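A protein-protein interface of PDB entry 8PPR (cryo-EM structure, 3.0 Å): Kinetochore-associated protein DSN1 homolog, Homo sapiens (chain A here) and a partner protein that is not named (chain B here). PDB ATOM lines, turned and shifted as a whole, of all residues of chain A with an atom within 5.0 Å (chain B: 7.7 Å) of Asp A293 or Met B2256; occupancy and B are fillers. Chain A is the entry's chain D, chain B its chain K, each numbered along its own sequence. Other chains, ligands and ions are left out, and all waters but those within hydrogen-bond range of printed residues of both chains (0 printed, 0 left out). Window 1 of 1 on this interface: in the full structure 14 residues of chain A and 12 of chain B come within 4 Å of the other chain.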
ATOM      1  N   GLU A 289      11.938 -32.064 -11.123  1.00  0.00           N
ATOM      2  CA  GLU A 289      10.671 -32.407 -11.764  1.00  0.00           C
ATOM      3  C   GLU A 289       9.635 -31.304 -11.570  1.00  0.00           C
ATOM      4  O   GLU A 289       8.860 -30.997 -12.485  1.00  0.00           O
ATOM      5  CB  GLU A 289      10.151 -33.736 -11.222  1.00  0.00           C
ATOM      6  CG  GLU A 289       8.873 -34.209 -11.889  1.00  0.00           C
ATOM      7  CD  GLU A 289       7.643 -33.903 -11.062  1.00  0.00           C
ATOM      8  OE1 GLU A 289       7.785 -33.259 -10.003  1.00  0.00           O
ATOM      9  OE2 GLU A 289       6.533 -34.305 -11.472  1.00  0.00           O
ATOM     10  N   LEU A 290       9.591 -30.710 -10.376  1.00  0.00           N
ATOM     11  CA  LEU A 290       8.660 -29.606 -10.140  1.00  0.00           C
ATOM     12  C   LEU A 290       8.977 -28.415 -11.035  1.00  0.00           C
ATOM     13  O   LEU A 290       8.071 -27.795 -11.613  1.00  0.00           O
ATOM     14  CB  LEU A 290       8.701 -29.190  -8.672  1.00  0.00           C
ATOM     15  CG  LEU A 290       8.196 -30.219  -7.666  1.00  0.00           C
ATOM     16  CD1 LEU A 290       8.009 -29.576  -6.305  1.00  0.00           C
ATOM     17  CD2 LEU A 290       6.898 -30.815  -8.162  1.00  0.00           C
ATOM     18  N   VAL A 291      10.262 -28.079 -11.161  1.00  0.00           N
ATOM     19  CA  VAL A 291      10.665 -27.007 -12.066  1.00  0.00           C
ATOM     20  C   VAL A 291      10.259 -27.349 -13.489  1.00  0.00           C
ATOM     21  O   VAL A 291       9.844 -26.481 -14.268  1.00  0.00           O
ATOM     22  CB  VAL A 291      12.181 -26.758 -11.956  1.00  0.00           C
ATOM     23  CG1 VAL A 291      12.673 -25.920 -13.128  1.00  0.00           C
ATOM     24  CG2 VAL A 291      12.513 -26.087 -10.634  1.00  0.00           C
ATOM     25  N   MET A 292      10.374 -28.624 -13.850  1.00  0.00           N
ATOM     26  CA  MET A 292       9.995 -29.056 -15.184  1.00  0.00           C
ATOM     27  C   MET A 292       8.505 -28.849 -15.424  1.00  0.00           C
ATOM     28  O   MET A 292       8.089 -28.412 -16.507  1.00  0.00           O
ATOM     29  CB  MET A 292      10.366 -30.524 -15.361  1.00  0.00           C
ATOM     30  CG  MET A 292      10.152 -30.957 -16.753  1.00  0.00           C
ATOM     31  SD  MET A 292      11.355 -30.001 -17.671  1.00  0.00           S
ATOM     32  CE  MET A 292      10.569 -30.018 -19.248  1.00  0.00           C
ATOM     33  N   ASP A 293       7.685 -29.167 -14.423  1.00  0.00           N
ATOM     34  CA  ASP A 293       6.250 -28.925 -14.533  1.00  0.00           C
ATOM     35  C   ASP A 293       5.968 -27.442 -14.716  1.00  0.00           C
ATOM     36  O   ASP A 293       5.118 -27.051 -15.528  1.00  0.00           O
ATOM     37  CB  ASP A 293       5.531 -29.457 -13.295  1.00  0.00           C
ATOM     38  CG  ASP A 293       5.737 -30.937 -13.094  1.00  0.00           C
ATOM     39  OD1 ASP A 293       6.346 -31.577 -13.978  1.00  0.00           O
ATOM     40  OD2 ASP A 293       5.313 -31.454 -12.041  1.00  0.00           O
ATOM     41  N   GLU A 294       6.672 -26.600 -13.956  1.00  0.00           N
ATOM     42  CA  GLU A 294       6.502 -25.157 -14.095  1.00  0.00           C
ATOM     43  C   GLU A 294       6.848 -24.695 -15.505  1.00  0.00           C
ATOM     44  O   GLU A 294       6.141 -23.861 -16.090  1.00  0.00           O
ATOM     45  CB  GLU A 294       7.373 -24.430 -13.070  1.00  0.00           C
ATOM     46  CG  GLU A 294       7.034 -22.959 -12.896  1.00  0.00           C
ATOM     47  CD  GLU A 294       7.395 -22.437 -11.517  1.00  0.00           C
ATOM     48  OE1 GLU A 294       7.220 -23.185 -10.533  1.00  0.00           O
ATOM     49  OE2 GLU A 294       7.854 -21.278 -11.418  1.00  0.00           O
ATOM     50  N   LEU A 295       7.939 -25.221 -16.062  1.00  0.00           N
ATOM     51  CA  LEU A 295       8.339 -24.860 -17.418  1.00  0.00           C
ATOM     52  C   LEU A 295       7.273 -25.258 -18.427  1.00  0.00           C
ATOM     53  O   LEU A 295       6.934 -24.481 -19.332  1.00  0.00           O
ATOM     54  CB  LEU A 295       9.666 -25.528 -17.762  1.00  0.00           C
ATOM     55  CG  LEU A 295      10.935 -24.717 -17.514  1.00  0.00           C
ATOM     56  CD1 LEU A 295      12.152 -25.628 -17.475  1.00  0.00           C
ATOM     57  CD2 LEU A 295      11.093 -23.642 -18.573  1.00  0.00           C
ATOM     58  N   GLN A 296       6.737 -26.472 -18.290  1.00  0.00           N
ATOM     59  CA  GLN A 296       5.694 -26.923 -19.205  1.00  0.00           C
ATOM     60  C   GLN A 296       4.468 -26.024 -19.120  1.00  0.00           C
ATOM     61  O   GLN A 296       3.879 -25.661 -20.147  1.00  0.00           O
ATOM     62  CB  GLN A 296       5.319 -28.370 -18.896  1.00  0.00           C
ATOM     63  CG  GLN A 296       6.139 -29.385 -19.661  1.00  0.00           C
ATOM     64  CD  GLN A 296       5.462 -30.731 -19.757  1.00  0.00           C
ATOM     65  OE1 GLN A 296       4.486 -31.000 -19.057  1.00  0.00           O
ATOM     66  NE2 GLN A 296       5.979 -31.591 -20.626  1.00  0.00           N
ATOM     67  N   GLY A 297       4.069 -25.657 -17.901  1.00  0.00           N
ATOM     68  CA  GLY A 297       2.928 -24.769 -17.747  1.00  0.00           C
ATOM     69  C   GLY A 297       3.156 -23.412 -18.383  1.00  0.00           C
ATOM     70  O   GLY A 297       2.261 -22.856 -19.029  1.00  0.00           O
ATOM     71  N   LYS A 300       2.845 -23.754 -22.133  1.00  0.00           N
ATOM     72  CA  LYS A 300       1.447 -23.891 -22.528  1.00  0.00           C
ATOM     73  C   LYS A 300       0.730 -22.547 -22.494  1.00  0.00           C
ATOM     74  O   LYS A 300      -0.047 -22.218 -23.406  1.00  0.00           O
ATOM     75  CB  LYS A 300       0.741 -24.886 -21.610  1.00  0.00           C
ATOM     76  CG  LYS A 300      -0.764 -24.910 -21.765  1.00  0.00           C
ATOM     77  CD  LYS A 300      -1.433 -24.937 -20.404  1.00  0.00           C
ATOM     78  CE  LYS A 300      -1.339 -26.309 -19.761  1.00  0.00           C
ATOM     79  NZ  LYS A 300      -2.201 -26.404 -18.551  1.00  0.00           N
ATOM     80  N   LEU B2246     -10.233 -22.153 -15.555  1.00  0.00           N
ATOM     81  CA  LEU B2246      -9.091 -22.778 -14.907  1.00  0.00           C
ATOM     82  C   LEU B2246      -8.246 -23.574 -15.887  1.00  0.00           C
ATOM     83  O   LEU B2246      -7.036 -23.701 -15.684  1.00  0.00           O
ATOM     84  CB  LEU B2246      -9.570 -23.677 -13.771  1.00  0.00           C
ATOM     85  CG  LEU B2246     -10.259 -22.936 -12.627  1.00  0.00           C
ATOM     86  CD1 LEU B2246     -10.630 -23.894 -11.509  1.00  0.00           C
ATOM     87  CD2 LEU B2246      -9.371 -21.815 -12.109  1.00  0.00           C
ATOM     88  N   LYS B2247      -8.854 -24.106 -16.945  1.00  0.00           N
ATOM     89  CA  LYS B2247      -8.081 -24.748 -17.996  1.00  0.00           C
ATOM     90  C   LYS B2247      -7.301 -23.738 -18.817  1.00  0.00           C
ATOM     91  O   LYS B2247      -6.328 -24.112 -19.480  1.00  0.00           O
ATOM     92  CB  LYS B2247      -8.999 -25.556 -18.914  1.00  0.00           C
ATOM     93  CG  LYS B2247      -9.481 -26.866 -18.318  1.00  0.00           C
ATOM     94  CD  LYS B2247      -9.840 -27.865 -19.406  1.00  0.00           C
ATOM     95  CE  LYS B2247     -10.259 -29.202 -18.814  1.00  0.00           C
ATOM     96  NZ  LYS B2247     -10.490 -30.232 -19.865  1.00  0.00           N
ATOM     97  N   GLY B2250      -4.978 -21.678 -15.388  1.00  0.00           N
ATOM     98  CA  GLY B2250      -4.535 -22.523 -14.304  1.00  0.00           C
ATOM     99  C   GLY B2250      -3.086 -22.334 -13.894  1.00  0.00           C
ATOM    100  O   GLY B2250      -2.780 -22.193 -12.705  1.00  0.00           O
ATOM    101  N   PRO B2251      -2.159 -22.341 -14.858  1.00  0.00           N
ATOM    102  CA  PRO B2251      -0.742 -22.169 -14.499  1.00  0.00           C
ATOM    103  C   PRO B2251      -0.434 -20.848 -13.824  1.00  0.00           C
ATOM    104  O   PRO B2251       0.563 -20.763 -13.096  1.00  0.00           O
ATOM    105  CB  PRO B2251      -0.027 -22.289 -15.849  1.00  0.00           C
ATOM    106  CG  PRO B2251      -0.907 -23.185 -16.634  1.00  0.00           C
ATOM    107  CD  PRO B2251      -2.306 -22.780 -16.258  1.00  0.00           C
ATOM    108  N   ASN B2252      -1.246 -19.811 -14.042  1.00  0.00           N
ATOM    109  CA  ASN B2252      -1.061 -18.572 -13.295  1.00  0.00           C
ATOM    110  C   ASN B2252      -1.257 -18.795 -11.803  1.00  0.00           C
ATOM    111  O   ASN B2252      -0.655 -18.093 -10.984  1.00  0.00           O
ATOM    112  CB  ASN B2252      -2.025 -17.500 -13.804  1.00  0.00           C
ATOM    113  CG  ASN B2252      -1.545 -16.844 -15.083  1.00  0.00           C
ATOM    114  OD1 ASN B2252      -0.715 -17.396 -15.805  1.00  0.00           O
ATOM    115  ND2 ASN B2252      -2.064 -15.654 -15.370  1.00  0.00           N
ATOM    116  N   TYR B2253      -2.087 -19.768 -11.435  1.00  0.00           N
ATOM    117  CA  TYR B2253      -2.336 -20.114 -10.045  1.00  0.00           C
ATOM    118  C   TYR B2253      -1.642 -21.405  -9.636  1.00  0.00           C
ATOM    119  O   TYR B2253      -2.059 -22.039  -8.663  1.00  0.00           O
ATOM    120  CB  TYR B2253      -3.838 -20.226  -9.798  1.00  0.00           C
ATOM    121  CG  TYR B2253      -4.566 -18.915  -9.959  1.00  0.00           C
ATOM    122  CD1 TYR B2253      -3.916 -17.710  -9.734  1.00  0.00           C
ATOM    123  CD2 TYR B2253      -5.898 -18.881 -10.343  1.00  0.00           C
ATOM    124  CE1 TYR B2253      -4.573 -16.507  -9.883  1.00  0.00           C
ATOM    125  CE2 TYR B2253      -6.566 -17.682 -10.494  1.00  0.00           C
ATOM    126  CZ  TYR B2253      -5.898 -16.499 -10.263  1.00  0.00           C
ATOM    127  OH  TYR B2253      -6.558 -15.301 -10.413  1.00  0.00           O
ATOM    128  N   ASN B2254      -0.613 -21.818 -10.378  1.00  0.00           N
ATOM    129  CA  ASN B2254       0.162 -23.035 -10.155  1.00  0.00           C
ATOM    130  C   ASN B2254      -0.646 -24.302 -10.392  1.00  0.00           C
ATOM    131  O   ASN B2254      -0.156 -25.403 -10.110  1.00  0.00           O
ATOM    132  CB  ASN B2254       0.775 -23.077  -8.751  1.00  0.00           C
ATOM    133  CG  ASN B2254       1.960 -22.153  -8.612  1.00  0.00           C
ATOM    134  OD1 ASN B2254       1.869 -21.098  -7.985  1.00  0.00           O
ATOM    135  ND2 ASN B2254       3.086 -22.543  -9.197  1.00  0.00           N
ATOM    136  N   LEU B2255      -1.867 -24.185 -10.903  1.00  0.00           N
ATOM    137  CA  LEU B2255      -2.693 -25.346 -11.218  1.00  0.00           C
ATOM    138  C   LEU B2255      -2.289 -25.844 -12.598  1.00  0.00           C
ATOM    139  O   LEU B2255      -2.742 -25.323 -13.619  1.00  0.00           O
ATOM    140  CB  LEU B2255      -4.171 -24.983 -11.164  1.00  0.00           C
ATOM    141  CG  LEU B2255      -5.156 -26.035 -11.667  1.00  0.00           C
ATOM    142  CD1 LEU B2255      -4.985 -27.341 -10.906  1.00  0.00           C
ATOM    143  CD2 LEU B2255      -6.571 -25.511 -11.536  1.00  0.00           C
ATOM    144  N   MET B2256      -1.425 -26.859 -12.635  1.00  0.00           N
ATOM    145  CA  MET B2256      -0.880 -27.311 -13.908  1.00  0.00           C
ATOM    146  C   MET B2256      -1.894 -28.083 -14.736  1.00  0.00           C
ATOM    147  O   MET B2256      -1.955 -27.901 -15.956  1.00  0.00           O
ATOM    148  CB  MET B2256       0.349 -28.190 -13.678  1.00  0.00           C
ATOM    149  CG  MET B2256       1.532 -27.476 -13.059  1.00  0.00           C
ATOM    150  SD  MET B2256       2.172 -26.130 -14.070  1.00  0.00           S
ATOM    151  CE  MET B2256       1.485 -24.714 -13.218  1.00  0.00           C
ATOM    152  N   ASN B2257      -2.699 -28.934 -14.107  1.00  0.00           N
ATOM    153  CA  ASN B2257      -3.531 -29.851 -14.866  1.00  0.00           C
ATOM    154  C   ASN B2257      -4.862 -30.056 -14.161  1.00  0.00           C
ATOM    155  O   ASN B2257      -4.947 -30.023 -12.931  1.00  0.00           O
ATOM    156  CB  ASN B2257      -2.828 -31.199 -15.065  1.00  0.00           C
ATOM    157  CG  ASN B2257      -3.713 -32.220 -15.745  1.00  0.00           C
ATOM    158  OD1 ASN B2257      -4.485 -31.888 -16.643  1.00  0.00           O
ATOM    159  ND2 ASN B2257      -3.612 -33.471 -15.315  1.00  0.00           N
ATOM    160  N   ILE B2258      -5.899 -30.267 -14.965  1.00  0.00           N
ATOM    161  CA  ILE B2258      -7.223 -30.640 -14.491  1.00  0.00           C
ATOM    162  C   ILE B2258      -7.686 -31.835 -15.310  1.00  0.00           C
ATOM    163  O   ILE B2258      -7.580 -31.827 -16.540  1.00  0.00           O
ATOM    164  CB  ILE B2258      -8.226 -29.480 -14.618  1.00  0.00           C
ATOM    165  CG1 ILE B2258      -7.920 -28.394 -13.589  1.00  0.00           C
ATOM    166  CG2 ILE B2258      -9.652 -29.982 -14.453  1.00  0.00           C
ATOM    167  CD1 ILE B2258      -8.871 -27.228 -13.658  1.00  0.00           C
ATOM    168  N   LEU B2267      -7.655 -31.733  -9.245  1.00  0.00           N
ATOM    169  CA  LEU B2267      -6.849 -30.535  -9.429  1.00  0.00           C
ATOM    170  C   LEU B2267      -5.407 -30.849  -9.055  1.00  0.00           C
ATOM    171  O   LEU B2267      -5.125 -31.227  -7.913  1.00  0.00           O
ATOM    172  CB  LEU B2267      -7.386 -29.382  -8.584  1.00  0.00           C
ATOM    173  CG  LEU B2267      -8.456 -28.483  -9.207  1.00  0.00           C
ATOM    174  CD1 LEU B2267      -9.605 -29.291  -9.784  1.00  0.00           C
ATOM    175  CD2 LEU B2267      -8.967 -27.484  -8.181  1.00  0.00           C
ATOM    176  N   LEU B2268      -4.498 -30.693 -10.012  1.00  0.00           N
ATOM    177  CA  LEU B2268      -3.085 -30.995  -9.807  1.00  0.00           C
ATOM    178  C   LEU B2268      -2.335 -29.686  -9.590  1.00  0.00           C
ATOM    179  O   LEU B2268      -2.083 -28.936 -10.535  1.00  0.00           O
ATOM    180  CB  LEU B2268      -2.514 -31.771 -10.986  1.00  0.00           C
ATOM    181  CG  LEU B2268      -1.013 -32.046 -10.882  1.00  0.00           C
ATOM    182  CD1 LEU B2268      -0.687 -32.761  -9.579  1.00  0.00           C
ATOM    183  CD2 LEU B2268      -0.532 -32.854 -12.075  1.00  0.00           C
ATOM    184  N   PHE B2269      -1.981 -29.418  -8.339  1.00  0.00           N
ATOM    185  CA  PHE B2269      -1.159 -28.269  -7.993  1.00  0.00           C
ATOM    186  C   PHE B2269       0.286 -28.713  -7.832  1.00  0.00           C
ATOM    187  O   PHE B2269       0.558 -29.740  -7.201  1.00  0.00           O
ATOM    188  CB  PHE B2269      -1.650 -27.616  -6.702  1.00  0.00           C
ATOM    189  CG  PHE B2269      -2.980 -26.943  -6.833  1.00  0.00           C
ATOM    190  CD1 PHE B2269      -4.149 -27.682  -6.828  1.00  0.00           C
ATOM    191  CD2 PHE B2269      -3.064 -25.567  -6.948  1.00  0.00           C
ATOM    192  CE1 PHE B2269      -5.375 -27.064  -6.943  1.00  0.00           C
ATOM    193  CE2 PHE B2269      -4.288 -24.941  -7.063  1.00  0.00           C
ATOM    194  CZ  PHE B2269      -5.445 -25.691  -7.061  1.00  0.00           C
ATOM    195  N   SER B2270       1.207 -27.947  -8.406  1.00  0.00           N
ATOM    196  CA  SER B2270       2.629 -28.192  -8.217  1.00  0.00           C
ATOM    197  C   SER B2270       3.366 -26.865  -8.258  1.00  0.00           C
ATOM    198  O   SER B2270       3.022 -25.984  -9.052  1.00  0.00           O
ATOM    199  CB  SER B2270       3.188 -29.139  -9.283  1.00  0.00           C
ATOM    200  OG  SER B2270       3.089 -28.570 -10.574  1.00  0.00           O
ATOM    201  N   SER B2271       4.369 -26.725  -7.397  1.00  0.00           N
ATOM    202  CA  SER B2271       5.199 -25.525  -7.376  1.00  0.00           C
ATOM    203  C   SER B2271       6.524 -25.880  -6.727  1.00  0.00           C
ATOM    204  O   SER B2271       6.544 -26.382  -5.599  1.00  0.00           O
ATOM    205  CB  SER B2271       4.515 -24.391  -6.616  1.00  0.00           C
ATOM    206  OG  SER B2271       5.449 -23.379  -6.282  1.00  0.00           O
ATOM    207  N   SER B2272       7.621 -25.621  -7.432  1.00  0.00           N
ATOM    208  CA  SER B2272       8.953 -25.854  -6.899  1.00  0.00           C
ATOM    209  C   SER B2272       9.373 -24.781  -5.910  1.00  0.00           C
ATOM    210  O   SER B2272      10.383 -24.950  -5.219  1.00  0.00           O
ATOM    211  CB  SER B2272       9.971 -25.930  -8.038  1.00  0.00           C
ATOM    212  OG  SER B2272      10.074 -24.686  -8.704  1.00  0.00           O
ATOM    213  N   ALA B2276       6.081 -28.263  -3.247  1.00  0.00           N
ATOM    214  CA  ALA B2276       4.802 -28.892  -2.958  1.00  0.00           C
ATOM    215  C   ALA B2276       4.130 -29.286  -4.263  1.00  0.00           C
ATOM    216  O   ALA B2276       3.999 -28.460  -5.172  1.00  0.00           O
ATOM    217  CB  ALA B2276       3.894 -27.958  -2.154  1.00  0.00           C
ATOM    218  N   LYS B2277       3.712 -30.545  -4.350  1.00  0.00           N
ATOM    219  CA  LYS B2277       2.943 -31.020  -5.493  1.00  0.00           C
ATOM    220  C   LYS B2277       1.940 -32.042  -4.991  1.00  0.00           C
ATOM    221  O   LYS B2277       2.324 -33.029  -4.356  1.00  0.00           O
ATOM    222  CB  LYS B2277       3.843 -31.632  -6.564  1.00  0.00           C
ATOM    223  CG  LYS B2277       3.104 -32.561  -7.509  1.00  0.00           C
ATOM    224  CD  LYS B2277       3.909 -32.830  -8.766  1.00  0.00           C
ATOM    225  CE  LYS B2277       3.277 -33.932  -9.597  1.00  0.00           C
ATOM    226  NZ  LYS B2277       3.876 -34.008 -10.958  1.00  0.00           N
ATOM    227  N   VAL B2301       4.464 -34.622  -3.850  1.00  0.00           N
ATOM    228  CA  VAL B2301       5.757 -34.110  -3.412  1.00  0.00           C
ATOM    229  C   VAL B2301       5.513 -33.052  -2.347  1.00  0.00           C
ATOM    230  O   VAL B2301       4.644 -32.189  -2.509  1.00  0.00           O
ATOM    231  CB  VAL B2301       6.567 -33.523  -4.587  1.00  0.00           C
ATOM    232  CG1 VAL B2301       7.653 -32.585  -4.084  1.00  0.00           C
ATOM    233  CG2 VAL B2301       7.171 -34.640  -5.423  1.00  0.00           C
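O of Ser B2271 touches CD1 of Leu A290 (3.6 Å).
Leu A290 touches Ser B2272 (CB to CB, 3.6 Å).
Ala B2276 touches Leu A290.
Leu A290 touches Lys B2277.
Val B2301 touches Leu A290.
Ser B2272 touches Val A291 (OG to CG2, 3.4 Å).
Ser B2270 touches Asp A293.
CB of Pro B2251 touches O of Gly A297, at 3.96 Å.
CA of Gly A297 touches SD of Met B2256, 3.99 Å away.
Lys A300 touches Pro B2251 (NZ to CG, 3.96 Å).
Printed residues of chain B within 4 Å of Asp A293: Met B2256, Ser B2270 and Lys B2277.
Printed residues of chain A within 4 Å of Met B2256: Asp A293, Gly A297 and Lys A300.
Printed residues of chain B within 4 Å of Leu A290: Ser B2271, Ser B2272, Ala B2276, Lys B2277 and Val B2301.
Of the printed residues of chain B, Gly A297 touches Pro B2251 (3.96 Å) and Met B2256 (3.99 Å).
Of the printed residues of chain A, Ser B2271 touches Leu A290.
Of the printed residues of chain B, Glu A294 touches Ser B2272 (3.7 Å).
Leu B2246 touches none of the printed residues of chain A.
The nearest printed residue of chain A that does not touch Met B2256 is Glu A294 (4.4 Å).
The nearest printed residue of chain A that does not touch Ser B2271 is Glu A294 (4.4 Å).
Hydrophobic or aromatic side chains of chain B within 4 Å of the printed part of chain A: Pro B2251, Met B2256 and Val B2301.
Hydrophobic or aromatic side chains of chain A within 4 Å of the printed part of chain B: Leu A290 and Val A291.
Among the printed residues, 15 pairs touch across the chains.
Among the printed residues, Asp or Glu carboxylates within 4 Å of a Lys or Arg side-chain nitrogen of the other chain: Glu A289 with Lys B2277 and Asp A293 with Lys B2277.
SD of Met B2256 sits close to O of Asp A293 (3.4 Å).
NZ of Lys B2277 is in salt-bridge range of OD2 of Asp A293 (3.1 Å).
The side-chain carboxylate (OE2) of Glu A289 lies within salt-bridge range of the side-chain amino group (NZ) of Lys B2277 (2.7 Å).
The backbone carbonyl oxygen of Met B2256 sits at hydrogen-bond distance from the side-chain amino group of Lys A300 (3.0 Å).
The backbone carbonyl oxygen (O) of Leu B2268 is in hydrogen-bond range of the backbone NH (N) of Met B2256 (3.0 Å).
O of Ala B2276 sits at hydrogen-bond distance from N of Ser B2271, at 2.8 Å.
The backbone carbonyl oxygen (O) of Asn B2254 sits at hydrogen-bond distance from the backbone NH (N) of Ser B2270, 3.4 Å away.
The backbone NH of Lys B2277 sits at hydrogen-bond distance from the backbone carbonyl oxygen of Val B2301, at 2.6 Å.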
